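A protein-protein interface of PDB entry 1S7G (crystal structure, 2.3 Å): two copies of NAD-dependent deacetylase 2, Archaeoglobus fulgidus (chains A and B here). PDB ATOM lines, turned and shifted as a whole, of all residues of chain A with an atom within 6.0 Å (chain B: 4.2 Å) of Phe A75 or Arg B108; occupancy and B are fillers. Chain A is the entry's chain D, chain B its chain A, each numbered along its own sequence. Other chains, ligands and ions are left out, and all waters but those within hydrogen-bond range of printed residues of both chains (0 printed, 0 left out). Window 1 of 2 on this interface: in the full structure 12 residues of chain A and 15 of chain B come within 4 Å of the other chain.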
ATOM      1  N   LYS A  73      15.517 -11.582  -2.866  1.00  0.00           N
ATOM      2  CA  LYS A  73      14.058 -11.541  -2.704  1.00  0.00           C
ATOM      3  C   LYS A  73      13.293 -11.069  -3.938  1.00  0.00           C
ATOM      4  O   LYS A  73      13.788 -10.253  -4.719  1.00  0.00           O
ATOM      5  CB  LYS A  73      13.693 -10.663  -1.506  1.00  0.00           C
ATOM      6  N   LEU A  74      12.076 -11.582  -4.094  1.00  0.00           N
ATOM      7  CA  LEU A  74      11.225 -11.235  -5.231  1.00  0.00           C
ATOM      8  C   LEU A  74      10.493  -9.913  -5.045  1.00  0.00           C
ATOM      9  O   LEU A  74      10.142  -9.532  -3.924  1.00  0.00           O
ATOM     10  CB  LEU A  74      10.195 -12.341  -5.483  1.00  0.00           C
ATOM     11  CG  LEU A  74      10.716 -13.690  -5.976  1.00  0.00           C
ATOM     12  CD1 LEU A  74       9.560 -14.674  -6.060  1.00  0.00           C
ATOM     13  CD2 LEU A  74      11.386 -13.523  -7.336  1.00  0.00           C
ATOM     14  N   PHE A  75      10.258  -9.226  -6.161  1.00  0.00           N
ATOM     15  CA  PHE A  75       9.558  -7.945  -6.166  1.00  0.00           C
ATOM     16  C   PHE A  75      10.246  -6.934  -5.253  1.00  0.00           C
ATOM     17  O   PHE A  75       9.596  -6.059  -4.674  1.00  0.00           O
ATOM     18  CB  PHE A  75       8.104  -8.142  -5.726  1.00  0.00           C
ATOM     19  CG  PHE A  75       7.425  -9.305  -6.390  1.00  0.00           C
ATOM     20  CD1 PHE A  75       7.443  -9.439  -7.778  1.00  0.00           C
ATOM     21  CD2 PHE A  75       6.772 -10.269  -5.631  1.00  0.00           C
ATOM     22  CE1 PHE A  75       6.821 -10.521  -8.399  1.00  0.00           C
ATOM     23  CE2 PHE A  75       6.146 -11.353  -6.242  1.00  0.00           C
ATOM     24  CZ  PHE A  75       6.172 -11.479  -7.631  1.00  0.00           C
ATOM     25  N   ALA A  76      11.565  -7.064  -5.137  1.00  0.00           N
ATOM     26  CA  ALA A  76      12.367  -6.182  -4.302  1.00  0.00           C
ATOM     27  C   ALA A  76      12.060  -4.713  -4.575  1.00  0.00           C
ATOM     28  O   ALA A  76      11.691  -4.335  -5.686  1.00  0.00           O
ATOM     29  CB  ALA A  76      13.848  -6.456  -4.534  1.00  0.00           C
ATOM     30  N   GLU A  77      12.228  -3.888  -3.550  1.00  0.00           N
ATOM     31  CA  GLU A  77      11.968  -2.465  -3.680  1.00  0.00           C
ATOM     32  C   GLU A  77      12.794  -1.651  -2.686  1.00  0.00           C
ATOM     33  O   GLU A  77      13.386  -2.198  -1.755  1.00  0.00           O
ATOM     34  CB  GLU A  77      10.466  -2.195  -3.486  1.00  0.00           C
ATOM     35  CG  GLU A  77       9.853  -2.871  -2.265  1.00  0.00           C
ATOM     36  CD  GLU A  77       8.341  -2.719  -2.204  1.00  0.00           C
ATOM     37  OE1 GLU A  77       7.858  -1.580  -2.033  1.00  0.00           O
ATOM     38  OE2 GLU A  77       7.633  -3.743  -2.334  1.00  0.00           O
ATOM     39  N   PRO A  78      12.865  -0.330  -2.890  1.00  0.00           N
ATOM     40  CA  PRO A  78      13.624   0.547  -1.995  1.00  0.00           C
ATOM     41  C   PRO A  78      13.030   0.463  -0.599  1.00  0.00           C
ATOM     42  O   PRO A  78      11.838   0.199  -0.452  1.00  0.00           O
ATOM     43  CB  PRO A  78      13.410   1.926  -2.603  1.00  0.00           C
ATOM     44  CG  PRO A  78      13.212   1.641  -4.042  1.00  0.00           C
ATOM     45  CD  PRO A  78      12.325   0.429  -4.029  1.00  0.00           C
ATOM     46  N   TYR A  83      14.115   6.126   0.501  1.00  0.00           N
ATOM     47  CA  TYR A  83      13.116   7.176   0.351  1.00  0.00           C
ATOM     48  C   TYR A  83      13.480   8.407   1.175  1.00  0.00           C
ATOM     49  O   TYR A  83      13.276   9.534   0.727  1.00  0.00           O
ATOM     50  CB  TYR A  83      11.722   6.657   0.723  1.00  0.00           C
ATOM     51  CG  TYR A  83      11.139   5.734  -0.328  1.00  0.00           C
ATOM     52  CD1 TYR A  83      10.956   4.377  -0.073  1.00  0.00           C
ATOM     53  CD2 TYR A  83      10.805   6.215  -1.596  1.00  0.00           C
ATOM     54  CE1 TYR A  83      10.458   3.519  -1.054  1.00  0.00           C
ATOM     55  CE2 TYR A  83      10.308   5.366  -2.587  1.00  0.00           C
ATOM     56  CZ  TYR A  83      10.138   4.022  -2.309  1.00  0.00           C
ATOM     57  OH  TYR A  83       9.660   3.177  -3.286  1.00  0.00           O
ATOM     58  N   LEU B  74       4.983 -11.753 -15.077  1.00  0.00           N
ATOM     59  CA  LEU B  74       4.801 -12.059 -13.661  1.00  0.00           C
ATOM     60  C   LEU B  74       5.795 -11.269 -12.816  1.00  0.00           C
ATOM     61  O   LEU B  74       5.559 -11.022 -11.631  1.00  0.00           O
ATOM     62  CB  LEU B  74       4.994 -13.557 -13.406  1.00  0.00           C
ATOM     63  CG  LEU B  74       3.943 -14.484 -14.022  1.00  0.00           C
ATOM     64  CD1 LEU B  74       4.385 -15.940 -13.897  1.00  0.00           C
ATOM     65  CD2 LEU B  74       2.604 -14.257 -13.331  1.00  0.00           C
ATOM     66  N   PHE B  75       6.908 -10.871 -13.421  1.00  0.00           N
ATOM     67  CA  PHE B  75       7.905 -10.115 -12.680  1.00  0.00           C
ATOM     68  C   PHE B  75       8.052  -8.692 -13.180  1.00  0.00           C
ATOM     69  O   PHE B  75       9.112  -8.077 -13.048  1.00  0.00           O
ATOM     70  CB  PHE B  75       9.250 -10.839 -12.703  1.00  0.00           C
ATOM     71  CG  PHE B  75       9.198 -12.200 -12.084  1.00  0.00           C
ATOM     72  CD1 PHE B  75       8.829 -13.308 -12.837  1.00  0.00           C
ATOM     73  CD2 PHE B  75       9.469 -12.369 -10.729  1.00  0.00           C
ATOM     74  CE1 PHE B  75       8.729 -14.567 -12.249  1.00  0.00           C
ATOM     75  CE2 PHE B  75       9.370 -13.624 -10.131  1.00  0.00           C
ATOM     76  CZ  PHE B  75       9.001 -14.725 -10.894  1.00  0.00           C
ATOM     77  N   ALA B  76       6.972  -8.168 -13.748  1.00  0.00           N
ATOM     78  CA  ALA B  76       6.966  -6.802 -14.246  1.00  0.00           C
ATOM     79  C   ALA B  76       7.373  -5.846 -13.123  1.00  0.00           C
ATOM     80  O   ALA B  76       7.177  -6.125 -11.933  1.00  0.00           O
ATOM     81  CB  ALA B  76       5.576  -6.441 -14.765  1.00  0.00           C
ATOM     82  N   GLU B  77       7.952  -4.722 -13.513  1.00  0.00           N
ATOM     83  CA  GLU B  77       8.379  -3.705 -12.566  1.00  0.00           C
ATOM     84  C   GLU B  77       7.670  -2.413 -12.934  1.00  0.00           C
ATOM     85  O   GLU B  77       7.268  -2.215 -14.085  1.00  0.00           O
ATOM     86  CB  GLU B  77       9.898  -3.505 -12.645  1.00  0.00           C
ATOM     87  CG  GLU B  77      10.690  -4.777 -12.386  1.00  0.00           C
ATOM     88  CD  GLU B  77      12.189  -4.589 -12.552  1.00  0.00           C
ATOM     89  OE1 GLU B  77      12.612  -4.078 -13.619  1.00  0.00           O
ATOM     90  OE2 GLU B  77      12.940  -4.964 -11.617  1.00  0.00           O
ATOM     91  N   MET B 104      -0.026  -4.365  -8.163  1.00  0.00           N
ATOM     92  CA  MET B 104       0.654  -3.706  -7.047  1.00  0.00           C
ATOM     93  C   MET B 104       1.868  -2.886  -7.454  1.00  0.00           C
ATOM     94  O   MET B 104       2.756  -2.635  -6.636  1.00  0.00           O
ATOM     95  CB  MET B 104       1.097  -4.740  -6.022  1.00  0.00           C
ATOM     96  CG  MET B 104      -0.033  -5.564  -5.462  1.00  0.00           C
ATOM     97  SD  MET B 104       0.609  -6.774  -4.321  1.00  0.00           S
ATOM     98  CE  MET B 104       0.993  -5.681  -2.861  1.00  0.00           C
ATOM     99  N   LEU B 105       1.915  -2.474  -8.713  1.00  0.00           N
ATOM    100  CA  LEU B 105       3.034  -1.688  -9.198  1.00  0.00           C
ATOM    101  C   LEU B 105       3.078  -0.292  -8.578  1.00  0.00           C
ATOM    102  O   LEU B 105       4.140   0.320  -8.497  1.00  0.00           O
ATOM    103  CB  LEU B 105       2.985  -1.612 -10.724  1.00  0.00           C
ATOM    104  CG  LEU B 105       3.159  -2.990 -11.373  1.00  0.00           C
ATOM    105  CD1 LEU B 105       3.147  -2.873 -12.894  1.00  0.00           C
ATOM    106  CD2 LEU B 105       4.482  -3.602 -10.899  1.00  0.00           C
ATOM    107  N   HIS B 106       1.933   0.219  -8.131  1.00  0.00           N
ATOM    108  CA  HIS B 106       1.917   1.543  -7.510  1.00  0.00           C
ATOM    109  C   HIS B 106       2.647   1.547  -6.171  1.00  0.00           C
ATOM    110  O   HIS B 106       3.407   2.468  -5.879  1.00  0.00           O
ATOM    111  CB  HIS B 106       0.483   2.029  -7.314  1.00  0.00           C
ATOM    112  CG  HIS B 106      -0.168   2.495  -8.576  1.00  0.00           C
ATOM    113  ND1 HIS B 106       0.254   3.617  -9.257  1.00  0.00           N
ATOM    114  CD2 HIS B 106      -1.187   1.973  -9.301  1.00  0.00           C
ATOM    115  CE1 HIS B 106      -0.477   3.765 -10.349  1.00  0.00           C
ATOM    116  NE2 HIS B 106      -1.357   2.782 -10.398  1.00  0.00           N
ATOM    117  N   GLN B 107       2.419   0.520  -5.358  1.00  0.00           N
ATOM    118  CA  GLN B 107       3.070   0.441  -4.055  1.00  0.00           C
ATOM    119  C   GLN B 107       4.568   0.210  -4.237  1.00  0.00           C
ATOM    120  O   GLN B 107       5.386   0.863  -3.589  1.00  0.00           O
ATOM    121  CB  GLN B 107       2.461  -0.683  -3.208  1.00  0.00           C
ATOM    122  CG  GLN B 107       0.968  -0.512  -2.917  1.00  0.00           C
ATOM    123  CD  GLN B 107       0.073  -1.181  -3.961  1.00  0.00           C
ATOM    124  OE1 GLN B 107       0.302  -1.068  -5.163  1.00  0.00           O
ATOM    125  NE2 GLN B 107      -0.957  -1.872  -3.496  1.00  0.00           N
ATOM    126  N   ARG B 108       4.924  -0.712  -5.125  1.00  0.00           N
ATOM    127  CA  ARG B 108       6.328  -1.001  -5.389  1.00  0.00           C
ATOM    128  C   ARG B 108       7.055   0.238  -5.904  1.00  0.00           C
ATOM    129  O   ARG B 108       8.275   0.332  -5.789  1.00  0.00           O
ATOM    130  CB  ARG B 108       6.455  -2.149  -6.400  1.00  0.00           C
ATOM    131  CG  ARG B 108       6.144  -3.515  -5.791  1.00  0.00           C
ATOM    132  CD  ARG B 108       6.026  -4.603  -6.844  1.00  0.00           C
ATOM    133  NE  ARG B 108       7.271  -4.815  -7.578  1.00  0.00           N
ATOM    134  CZ  ARG B 108       7.409  -5.686  -8.574  1.00  0.00           C
ATOM    135  NH1 ARG B 108       8.579  -5.818  -9.187  1.00  0.00           N
ATOM    136  NH2 ARG B 108       6.376  -6.427  -8.961  1.00  0.00           N
ATOM    137  N   ALA B 109       6.311   1.190  -6.464  1.00  0.00           N
ATOM    138  CA  ALA B 109       6.923   2.412  -6.974  1.00  0.00           C
ATOM    139  C   ALA B 109       6.979   3.525  -5.920  1.00  0.00           C
ATOM    140  O   ALA B 109       7.500   4.603  -6.188  1.00  0.00           O
ATOM    141  CB  ALA B 109       6.182   2.902  -8.213  1.00  0.00           C
ATOM    142  N   GLY B 110       6.437   3.276  -4.731  1.00  0.00           N
ATOM    143  CA  GLY B 110       6.492   4.293  -3.693  1.00  0.00           C
ATOM    144  C   GLY B 110       5.187   4.923  -3.224  1.00  0.00           C
ATOM    145  O   GLY B 110       5.183   5.670  -2.247  1.00  0.00           O
ATOM    146  N   TRP B 135       2.013 -14.241  -2.565  1.00  0.00           N
ATOM    147  CA  TRP B 135       2.113 -14.707  -3.943  1.00  0.00           C
ATOM    148  C   TRP B 135       3.558 -15.084  -4.284  1.00  0.00           C
ATOM    149  O   TRP B 135       3.805 -15.916  -5.156  1.00  0.00           O
ATOM    150  CB  TRP B 135       1.628 -13.610  -4.881  1.00  0.00           C
ATOM    151  CG  TRP B 135       1.798 -13.909  -6.329  1.00  0.00           C
ATOM    152  CD1 TRP B 135       2.420 -13.121  -7.251  1.00  0.00           C
ATOM    153  CD2 TRP B 135       1.275 -15.032  -7.047  1.00  0.00           C
ATOM    154  NE1 TRP B 135       2.313 -13.680  -8.500  1.00  0.00           N
ATOM    155  CE2 TRP B 135       1.615 -14.853  -8.406  1.00  0.00           C
ATOM    156  CE3 TRP B 135       0.552 -16.168  -6.677  1.00  0.00           C
ATOM    157  CZ2 TRP B 135       1.255 -15.766  -9.398  1.00  0.00           C
ATOM    158  CZ3 TRP B 135       0.193 -17.085  -7.668  1.00  0.00           C
ATOM    159  CH2 TRP B 135       0.548 -16.875  -9.010  1.00  0.00           C
ATOM    160  N   SER B 136       4.510 -14.477  -3.585  1.00  0.00           N
ATOM    161  CA  SER B 136       5.923 -14.757  -3.830  1.00  0.00           C
ATOM    162  C   SER B 136       6.291 -16.216  -3.556  1.00  0.00           C
ATOM    163  O   SER B 136       7.313 -16.697  -4.040  1.00  0.00           O
ATOM    164  CB  SER B 136       6.810 -13.836  -2.979  1.00  0.00           C
ATOM    165  OG  SER B 136       6.633 -14.075  -1.593  1.00  0.00           O
ATOM    166  N   VAL B 139       4.770 -17.906  -7.163  1.00  0.00           N
ATOM    167  CA  VAL B 139       5.110 -17.376  -8.483  1.00  0.00           C
ATOM    168  C   VAL B 139       5.913 -18.295  -9.390  1.00  0.00           C
ATOM    169  O   VAL B 139       5.476 -18.626 -10.495  1.00  0.00           O
ATOM    170  CB  VAL B 139       5.872 -16.037  -8.388  1.00  0.00           C
ATOM    171  CG1 VAL B 139       4.965 -14.908  -8.807  1.00  0.00           C
ATOM    172  CG2 VAL B 139       6.387 -15.823  -6.981  1.00  0.00           C
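Of the 14 printed residues of chain B, 8 touch a printed residue of chain A. Printed residues of chain B that touch a printed residue of chain A: Leu B74, Phe B75, Gln B107, Arg B108, Ala B109, Gly B110, Ser B136 and Val B139. Along chain B the printed residues that touch a printed residue of chain A span positions 74 to 139. Of the 7 printed residues of chain A, 4 touch a printed residue of chain B. Printed residues of chain A that touch a printed residue of chain B: Leu A74, Phe A75, Glu A77 and Tyr A83. Hydrophobic or aromatic side chains of chain A that line the printed part of chain B: Leu A74, Phe A75 and Tyr A83. Among the printed residues, 11 pairs touch across the chains.
Leu A74 touches Phe B75, and with the chains exchanged Phe A75 touches Leu B74. Phe B75 touches its own counterpart, Phe A75. Positions printed for both chains: 74, 75, 76 and 77. Of the 11 pairs that touch across the chains among the printed residues, 3 have their exchanged pair printed and touching as well.
The backbone carbonyl oxygen (O) of Met B104 lies close to the side-chain amide oxygen (OE1) of Gln B107 (3.3 Å). The backbone carbonyl oxygen of Ala B76 is in hydrogen-bond range of the guanidinium group of Arg B108, at 3.1 Å.
Printed residues of chain B within 4 Å of Leu A74: Phe B75 (3.4 Å), Ser B136 (3.6 Å) and Val B139 (3.5 Å). Of the printed residues of chain B, Phe A75 touches Leu B74, Phe B75, Arg B108 and Val B139. Printed residues of chain A within 4 Å of Leu B74: Phe A75 (3.5 Å). The nearest residue of chain A that does not touch Arg B108 is Tyr A83 (4.03 Å).
Leu A74 touches Phe B75 (CD2 to CE2, 3.4 Å). Ser B136 touches Leu A74 (O to CD1, 3.6 Å). CD1 of Leu A74 touches CG2 of Val B139 (3.5 Å). Leu B74 touches Phe A75. Phe B75 touches Phe A75. CD1 of Phe A75 touches NH2 of Arg B108 (3.4 Å). Val B139 touches Phe A75. Glu A77 touches Gln B107 (OE1 to O, 3.8 Å). C of Ala B109 touches OH of Tyr A83 (3.8 Å). Gly B110 touches Tyr A83.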
